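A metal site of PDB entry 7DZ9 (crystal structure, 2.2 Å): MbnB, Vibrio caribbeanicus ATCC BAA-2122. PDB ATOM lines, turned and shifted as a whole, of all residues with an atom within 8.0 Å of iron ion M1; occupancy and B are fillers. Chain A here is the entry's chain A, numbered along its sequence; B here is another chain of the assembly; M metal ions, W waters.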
ATOM      1  N   HIS A  55     -18.623 -33.761 -20.426  1.00  0.00           N
ATOM      2  CA  HIS A  55     -17.812 -32.581 -20.676  1.00  0.00           C
ATOM      3  C   HIS A  55     -18.319 -31.955 -21.972  1.00  0.00           C
ATOM      4  O   HIS A  55     -18.335 -32.616 -22.999  1.00  0.00           O
ATOM      5  CB  HIS A  55     -16.347 -32.986 -20.804  1.00  0.00           C
ATOM      6  CG  HIS A  55     -15.373 -31.856 -20.693  1.00  0.00           C
ATOM      7  ND1 HIS A  55     -15.474 -30.867 -19.737  1.00  0.00           N
ATOM      8  CD2 HIS A  55     -14.236 -31.607 -21.382  1.00  0.00           C
ATOM      9  CE1 HIS A  55     -14.461 -30.027 -19.874  1.00  0.00           C
ATOM     10  NE2 HIS A  55     -13.691 -30.454 -20.859  1.00  0.00           N
ATOM     11  N   HIS A  91     -16.986 -25.210 -20.507  1.00  0.00           N
ATOM     12  CA  HIS A  91     -15.798 -24.370 -20.556  1.00  0.00           C
ATOM     13  C   HIS A  91     -16.161 -22.901 -20.459  1.00  0.00           C
ATOM     14  O   HIS A  91     -17.286 -22.493 -20.752  1.00  0.00           O
ATOM     15  CB  HIS A  91     -15.041 -24.569 -21.874  1.00  0.00           C
ATOM     16  CG  HIS A  91     -14.515 -25.954 -22.054  1.00  0.00           C
ATOM     17  ND1 HIS A  91     -15.317 -27.010 -22.427  1.00  0.00           N
ATOM     18  CD2 HIS A  91     -13.270 -26.463 -21.887  1.00  0.00           C
ATOM     19  CE1 HIS A  91     -14.579 -28.108 -22.498  1.00  0.00           C
ATOM     20  NE2 HIS A  91     -13.337 -27.801 -22.181  1.00  0.00           N
ATOM     21  N   GLU A 135     -14.542 -25.496 -16.275  1.00  0.00           N
ATOM     22  CA  GLU A 135     -13.125 -25.837 -16.278  1.00  0.00           C
ATOM     23  C   GLU A 135     -12.248 -24.598 -16.429  1.00  0.00           C
ATOM     24  O   GLU A 135     -12.546 -23.694 -17.223  1.00  0.00           O
ATOM     25  CB  GLU A 135     -12.811 -26.825 -17.410  1.00  0.00           C
ATOM     26  CG  GLU A 135     -11.362 -27.246 -17.453  1.00  0.00           C
ATOM     27  CD  GLU A 135     -11.047 -28.233 -18.586  1.00  0.00           C
ATOM     28  OE1 GLU A 135     -11.904 -28.425 -19.457  1.00  0.00           O
ATOM     29  OE2 GLU A 135      -9.924 -28.780 -18.597  1.00  0.00           O
ATOM     30  N   ASN A 136     -11.150 -24.547 -15.666  1.00  0.00           N
ATOM     31  CA  ASN A 136     -10.158 -23.476 -15.817  1.00  0.00           C
ATOM     32  C   ASN A 136      -9.412 -23.595 -17.135  1.00  0.00           C
ATOM     33  O   ASN A 136      -9.065 -24.690 -17.586  1.00  0.00           O
ATOM     34  CB  ASN A 136      -9.173 -23.483 -14.643  1.00  0.00           C
ATOM     35  CG  ASN A 136      -8.519 -24.846 -14.417  1.00  0.00           C
ATOM     36  OD1 ASN A 136      -9.204 -25.848 -14.205  1.00  0.00           O
ATOM     37  ND2 ASN A 136      -7.179 -24.881 -14.441  1.00  0.00           N
ATOM     38  N   TYR A 137      -9.133 -22.432 -17.750  1.00  0.00           N
ATOM     39  CA  TYR A 137      -8.484 -22.240 -19.036  1.00  0.00           C
ATOM     40  C   TYR A 137      -6.967 -22.244 -18.869  1.00  0.00           C
ATOM     41  O   TYR A 137      -6.448 -21.661 -17.926  1.00  0.00           O
ATOM     42  CB  TYR A 137      -8.914 -20.907 -19.665  1.00  0.00           C
ATOM     43  CG  TYR A 137      -8.539 -20.827 -21.121  1.00  0.00           C
ATOM     44  CD1 TYR A 137      -7.249 -20.441 -21.513  1.00  0.00           C
ATOM     45  CD2 TYR A 137      -9.438 -21.195 -22.117  1.00  0.00           C
ATOM     46  CE1 TYR A 137      -6.857 -20.422 -22.841  1.00  0.00           C
ATOM     47  CE2 TYR A 137      -9.068 -21.147 -23.468  1.00  0.00           C
ATOM     48  CZ  TYR A 137      -7.776 -20.755 -23.817  1.00  0.00           C
ATOM     49  OH  TYR A 137      -7.386 -20.713 -25.146  1.00  0.00           O
ATOM     50  N   PRO A 138      -6.241 -22.871 -19.800  1.00  0.00           N
ATOM     51  CA  PRO A 138      -4.754 -22.839 -19.775  1.00  0.00           C
ATOM     52  C   PRO A 138      -4.220 -21.541 -20.356  1.00  0.00           C
ATOM     53  O   PRO A 138      -3.772 -21.449 -21.512  1.00  0.00           O
ATOM     54  CB  PRO A 138      -4.392 -24.059 -20.644  1.00  0.00           C
ATOM     55  CG  PRO A 138      -5.510 -24.074 -21.703  1.00  0.00           C
ATOM     56  CD  PRO A 138      -6.760 -23.700 -20.906  1.00  0.00           C
ATOM     57  N   ASP A 165      -8.546 -28.408 -13.771  1.00  0.00           N
ATOM     58  CA  ASP A 165      -7.597 -29.050 -14.650  1.00  0.00           C
ATOM     59  C   ASP A 165      -6.200 -28.711 -14.149  1.00  0.00           C
ATOM     60  O   ASP A 165      -5.768 -27.558 -14.210  1.00  0.00           O
ATOM     61  CB  ASP A 165      -7.802 -28.611 -16.103  1.00  0.00           C
ATOM     62  CG  ASP A 165      -7.011 -29.459 -17.106  1.00  0.00           C
ATOM     63  OD1 ASP A 165      -5.782 -29.583 -16.952  1.00  0.00           O
ATOM     64  OD2 ASP A 165      -7.610 -29.979 -18.073  1.00  0.00           O
ATOM     65  N   ILE A 166      -5.507 -29.734 -13.648  1.00  0.00           N
ATOM     66  CA  ILE A 166      -4.220 -29.548 -12.990  1.00  0.00           C
ATOM     67  C   ILE A 166      -3.156 -29.085 -13.970  1.00  0.00           C
ATOM     68  O   ILE A 166      -2.331 -28.213 -13.656  1.00  0.00           O
ATOM     69  CB  ILE A 166      -3.819 -30.854 -12.285  1.00  0.00           C
ATOM     70  CG1 ILE A 166      -4.836 -31.180 -11.166  1.00  0.00           C
ATOM     71  CG2 ILE A 166      -2.391 -30.767 -11.763  1.00  0.00           C
ATOM     72  CD1 ILE A 166      -4.540 -32.473 -10.431  1.00  0.00           C
ATOM     73  N   SER A 167      -3.126 -29.655 -15.177  1.00  0.00           N
ATOM     74  CA  SER A 167      -2.094 -29.242 -16.110  1.00  0.00           C
ATOM     75  C   SER A 167      -2.438 -27.911 -16.778  1.00  0.00           C
ATOM     76  O   SER A 167      -1.521 -27.157 -17.116  1.00  0.00           O
ATOM     77  CB  SER A 167      -1.824 -30.339 -17.156  1.00  0.00           C
ATOM     78  OG  SER A 167      -3.006 -30.806 -17.798  1.00  0.00           O
ATOM     79  N   ASN A 168      -3.732 -27.588 -16.965  1.00  0.00           N
ATOM     80  CA  ASN A 168      -4.098 -26.244 -17.406  1.00  0.00           C
ATOM     81  C   ASN A 168      -3.573 -25.183 -16.455  1.00  0.00           C
ATOM     82  O   ASN A 168      -3.065 -24.146 -16.884  1.00  0.00           O
ATOM     83  CB  ASN A 168      -5.619 -26.103 -17.512  1.00  0.00           C
ATOM     84  CG  ASN A 168      -6.202 -26.891 -18.658  1.00  0.00           C
ATOM     85  OD1 ASN A 168      -5.517 -27.693 -19.292  1.00  0.00           O
ATOM     86  ND2 ASN A 168      -7.498 -26.704 -18.882  1.00  0.00           N
ATOM     87  N   ALA A 169      -3.712 -25.426 -15.158  1.00  0.00           N
ATOM     88  CA  ALA A 169      -3.216 -24.465 -14.171  1.00  0.00           C
ATOM     89  C   ALA A 169      -1.690 -24.413 -14.181  1.00  0.00           C
ATOM     90  O   ALA A 169      -1.105 -23.345 -13.972  1.00  0.00           O
ATOM     91  CB  ALA A 169      -3.745 -24.838 -12.780  1.00  0.00           C
ATOM     92  N   ILE A 171       0.075 -24.942 -16.922  1.00  0.00           N
ATOM     93  CA  ILE A 171       0.375 -24.180 -18.137  1.00  0.00           C
ATOM     94  C   ILE A 171       0.288 -22.685 -17.888  1.00  0.00           C
ATOM     95  O   ILE A 171       1.120 -21.910 -18.378  1.00  0.00           O
ATOM     96  CB  ILE A 171      -0.560 -24.603 -19.282  1.00  0.00           C
ATOM     97  CG1 ILE A 171      -0.195 -25.996 -19.801  1.00  0.00           C
ATOM     98  CG2 ILE A 171      -0.474 -23.608 -20.422  1.00  0.00           C
ATOM     99  CD1 ILE A 171      -1.282 -26.596 -20.707  1.00  0.00           C
ATOM    100  N   HIS A 194      -8.989 -32.887 -13.915  1.00  0.00           N
ATOM    101  CA  HIS A 194      -8.352 -33.266 -15.172  1.00  0.00           C
ATOM    102  C   HIS A 194      -6.835 -33.208 -15.015  1.00  0.00           C
ATOM    103  O   HIS A 194      -6.290 -32.392 -14.266  1.00  0.00           O
ATOM    104  CB  HIS A 194      -8.730 -32.305 -16.316  1.00  0.00           C
ATOM    105  CG  HIS A 194     -10.079 -32.514 -16.928  1.00  0.00           C
ATOM    106  ND1 HIS A 194     -10.485 -31.811 -18.043  1.00  0.00           N
ATOM    107  CD2 HIS A 194     -11.121 -33.308 -16.591  1.00  0.00           C
ATOM    108  CE1 HIS A 194     -11.712 -32.180 -18.368  1.00  0.00           C
ATOM    109  NE2 HIS A 194     -12.118 -33.089 -17.504  1.00  0.00           N
ATOM    110  N   ILE A 195      -6.123 -34.006 -15.807  1.00  0.00           N
ATOM    111  CA  ILE A 195      -4.672 -33.893 -15.894  1.00  0.00           C
ATOM    112  C   ILE A 195      -4.240 -34.441 -17.237  1.00  0.00           C
ATOM    113  O   ILE A 195      -4.818 -35.421 -17.734  1.00  0.00           O
ATOM    114  CB  ILE A 195      -3.983 -34.604 -14.707  1.00  0.00           C
ATOM    115  CG1 ILE A 195      -2.531 -34.124 -14.527  1.00  0.00           C
ATOM    116  CG2 ILE A 195      -4.046 -36.133 -14.850  1.00  0.00           C
ATOM    117  CD1 ILE A 195      -1.817 -34.792 -13.329  1.00  0.00           C
ATOM    118  N   ALA A 196      -3.241 -33.815 -17.839  1.00  0.00           N
ATOM    119  CA  ALA A 196      -2.845 -34.166 -19.203  1.00  0.00           C
ATOM    120  C   ALA A 196      -1.424 -33.686 -19.486  1.00  0.00           C
ATOM    121  O   ALA A 196      -0.765 -33.083 -18.635  1.00  0.00           O
ATOM    122  CB  ALA A 196      -3.811 -33.570 -20.230  1.00  0.00           C
ATOM    123  N   GLY A 197      -0.958 -33.995 -20.691  1.00  0.00           N
ATOM    124  CA  GLY A 197       0.298 -33.492 -21.188  1.00  0.00           C
ATOM    125  C   GLY A 197       0.109 -32.290 -22.111  1.00  0.00           C
ATOM    126  O   GLY A 197      -1.009 -31.883 -22.428  1.00  0.00           O
ATOM    127  N   PHE A 198       1.237 -31.749 -22.556  1.00  0.00           N
ATOM    128  CA  PHE A 198       1.250 -30.525 -23.349  1.00  0.00           C
ATOM    129  C   PHE A 198       2.521 -30.512 -24.188  1.00  0.00           C
ATOM    130  O   PHE A 198       3.353 -31.428 -24.121  1.00  0.00           O
ATOM    131  CB  PHE A 198       1.144 -29.301 -22.440  1.00  0.00           C
ATOM    132  CG  PHE A 198       2.099 -29.311 -21.263  1.00  0.00           C
ATOM    133  CD1 PHE A 198       3.463 -29.130 -21.444  1.00  0.00           C
ATOM    134  CD2 PHE A 198       1.618 -29.494 -19.975  1.00  0.00           C
ATOM    135  CE1 PHE A 198       4.343 -29.142 -20.364  1.00  0.00           C
ATOM    136  CE2 PHE A 198       2.498 -29.511 -18.878  1.00  0.00           C
ATOM    137  CZ  PHE A 198       3.866 -29.339 -19.079  1.00  0.00           C
ATOM    138  N   VAL A 208       1.471 -25.185 -24.953  1.00  0.00           N
ATOM    139  CA  VAL A 208       0.222 -25.392 -25.669  1.00  0.00           C
ATOM    140  C   VAL A 208      -0.488 -26.604 -25.049  1.00  0.00           C
ATOM    141  O   VAL A 208       0.136 -27.651 -24.823  1.00  0.00           O
ATOM    142  CB  VAL A 208       0.462 -25.616 -27.181  1.00  0.00           C
ATOM    143  CG1 VAL A 208      -0.869 -25.601 -27.961  1.00  0.00           C
ATOM    144  CG2 VAL A 208       1.437 -24.555 -27.731  1.00  0.00           C
ATOM    145  N   ASP A 209      -1.791 -26.456 -24.791  1.00  0.00           N
ATOM    146  CA  ASP A 209      -2.568 -27.458 -24.048  1.00  0.00           C
ATOM    147  C   ASP A 209      -3.098 -28.543 -25.005  1.00  0.00           C
ATOM    148  O   ASP A 209      -4.297 -28.666 -25.232  1.00  0.00           O
ATOM    149  CB  ASP A 209      -3.710 -26.796 -23.301  1.00  0.00           C
ATOM    150  CG  ASP A 209      -4.485 -27.771 -22.440  1.00  0.00           C
ATOM    151  OD1 ASP A 209      -3.863 -28.724 -21.914  1.00  0.00           O
ATOM    152  OD2 ASP A 209      -5.709 -27.616 -22.308  1.00  0.00           O
ATOM    153  N   THR A 210      -2.162 -29.369 -25.512  1.00  0.00           N
ATOM    154  CA  THR A 210      -2.450 -30.264 -26.632  1.00  0.00           C
ATOM    155  C   THR A 210      -3.080 -31.589 -26.213  1.00  0.00           C
ATOM    156  O   THR A 210      -3.681 -32.254 -27.077  1.00  0.00           O
ATOM    157  CB  THR A 210      -1.163 -30.602 -27.402  1.00  0.00           C
ATOM    158  OG1 THR A 210      -0.240 -31.185 -26.497  1.00  0.00           O
ATOM    159  CG2 THR A 210      -0.547 -29.359 -28.023  1.00  0.00           C
ATOM    160  N   HIS A 211      -2.908 -32.023 -24.973  1.00  0.00           N
ATOM    161  CA  HIS A 211      -3.324 -33.361 -24.557  1.00  0.00           C
ATOM    162  C   HIS A 211      -2.729 -34.442 -25.476  1.00  0.00           C
ATOM    163  O   HIS A 211      -3.398 -35.387 -25.885  1.00  0.00           O
ATOM    164  CB  HIS A 211      -4.849 -33.475 -24.507  1.00  0.00           C
ATOM    165  CG  HIS A 211      -5.514 -32.440 -23.654  1.00  0.00           C
ATOM    166  ND1 HIS A 211      -6.868 -32.176 -23.696  1.00  0.00           N
ATOM    167  CD2 HIS A 211      -5.005 -31.575 -22.729  1.00  0.00           C
ATOM    168  CE1 HIS A 211      -7.167 -31.220 -22.843  1.00  0.00           C
ATOM    169  NE2 HIS A 211      -6.054 -30.834 -22.245  1.00  0.00           N
ATOM    170  N   GLU A 238      -6.376 -37.002 -19.636  1.00  0.00           N
ATOM    171  CA  GLU A 238      -6.856 -36.639 -20.967  1.00  0.00           C
ATOM    172  C   GLU A 238      -5.879 -37.004 -22.067  1.00  0.00           C
ATOM    173  O   GLU A 238      -4.668 -36.922 -21.879  1.00  0.00           O
ATOM    174  CB  GLU A 238      -7.143 -35.137 -21.044  1.00  0.00           C
ATOM    175  CG  GLU A 238      -7.970 -34.589 -19.903  1.00  0.00           C
ATOM    176  CD  GLU A 238      -8.556 -33.232 -20.241  1.00  0.00           C
ATOM    177  OE1 GLU A 238      -7.964 -32.218 -19.814  1.00  0.00           O
ATOM    178  OE2 GLU A 238      -9.606 -33.174 -20.908  1.00  0.00           O
ATOM    179  N   ASP A 240      -5.937 -36.499 -26.575  1.00  0.00           N
ATOM    180  CA  ASP A 240      -6.652 -36.157 -27.812  1.00  0.00           C
ATOM    181  C   ASP A 240      -5.820 -36.382 -29.074  1.00  0.00           C
ATOM    182  O   ASP A 240      -6.374 -36.237 -30.173  1.00  0.00           O
ATOM    183  CB  ASP A 240      -7.135 -34.693 -27.791  1.00  0.00           C
ATOM    184  CG  ASP A 240      -8.165 -34.437 -26.687  1.00  0.00           C
ATOM    185  OD1 ASP A 240      -9.024 -35.315 -26.429  1.00  0.00           O
ATOM    186  OD2 ASP A 240      -8.111 -33.344 -26.087  1.00  0.00           O
ATOM    187  N   CYS B  18     -10.729 -31.093 -26.845  1.00  0.00           N
ATOM    188  CA  CYS B  18     -10.242 -30.064 -25.937  1.00  0.00           C
ATOM    189  C   CYS B  18      -8.786 -29.724 -26.192  1.00  0.00           C
ATOM    190  O   CYS B  18      -8.379 -28.579 -25.972  1.00  0.00           O
ATOM    191  CB  CYS B  18     -10.373 -30.542 -24.486  1.00  0.00           C
ATOM    192  SG  CYS B  18     -11.979 -30.366 -23.763  1.00  0.00           S
ATOM    193  N   GLY B  19      -8.024 -30.676 -26.722  1.00  0.00           N
ATOM    194  CA  GLY B  19      -6.648 -30.457 -27.095  1.00  0.00           C
ATOM    195  C   GLY B  19      -6.479 -29.362 -28.115  1.00  0.00           C
ATOM    196  O   GLY B  19      -7.067 -29.406 -29.204  1.00  0.00           O
ATOM    197  N   ALA B  20      -5.691 -28.339 -27.750  1.00  0.00           N
ATOM    198  CA  ALA B  20      -5.335 -27.285 -28.689  1.00  0.00           C
ATOM    199  C   ALA B  20      -4.394 -27.816 -29.781  1.00  0.00           C
ATOM    200  O   ALA B  20      -3.694 -28.812 -29.606  1.00  0.00           O
ATOM    201  CB  ALA B  20      -4.663 -26.132 -27.943  1.00  0.00           C
HETATM  202 FE    FE M   1      -6.003 -29.209 -20.855  1.00  0.00          FE
HETATM  203 FE    FE M   2      -9.121 -30.407 -19.315  1.00  0.00          FE
HETATM  204 FE    FE M   3     -11.818 -29.293 -21.447  1.00  0.00          FE
HETATM  205  O   HOH W   1      -5.368 -30.851 -19.514  1.00  0.00           O
HETATM  206  O   HOH W   2      -8.211 -29.096 -20.515  1.00  0.00           O
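Water W1 bridges the side-chain carboxylate of Asp 165 and the side-chain hydroxyl of Ser 167.
OD2 of Asp 165 touches iron ion M1, at 3.3 Å. OE1 of Glu 238 touches iron ion M1, at 3.7 Å. Of the 26 residues printed, 5 come within 4 Å of iron ion M1. Along chain A the residues within 4 Å of iron ion M1 span positions 165 to 238. The nearest printed residue that does not touch iron ion M1 is Glu 135 (4.5 Å).
N of His 211 sits at hydrogen-bond distance from O of Gly 197 (3.2 Å). O of His 211 is in hydrogen-bond range of N of Asp 240 (2.9 Å). N of Ala 20 of chain B lies within hydrogen-bond range of O of Asp 209, at 2.9 Å. The side-chain carboxylate (OD1) of Asp 165 lies within hydrogen-bond range of the backbone NH (N) of Asn 168, 2.9 Å away. The side-chain amide nitrogen (ND2) of Asn 168 sits close to the side-chain carboxylate (OE2) of Glu 135 (3.2 Å). The backbone carbonyl oxygen (O) of Asn 136 lies within hydrogen-bond range of the side-chain amide nitrogen (ND2) of Asn 168 (2.9 Å). The side-chain carboxylate (OD1) of Asp 165 is in hydrogen-bond range of the side-chain hydroxyl (OG) of Ser 167. O of Ile 195 lies within hydrogen-bond range of N of Glu 238 (2.9 Å).
Iron ion M1 is bound by NE2 of His 211 (2.1 Å), OD2 of Asp 209 (2.2 Å), water W1 (2.2 Å), OD1 of Asn 168 (2.2 Å), water W2 (2.2 Å) and OD1 of Asp 209 (2.4 Å).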
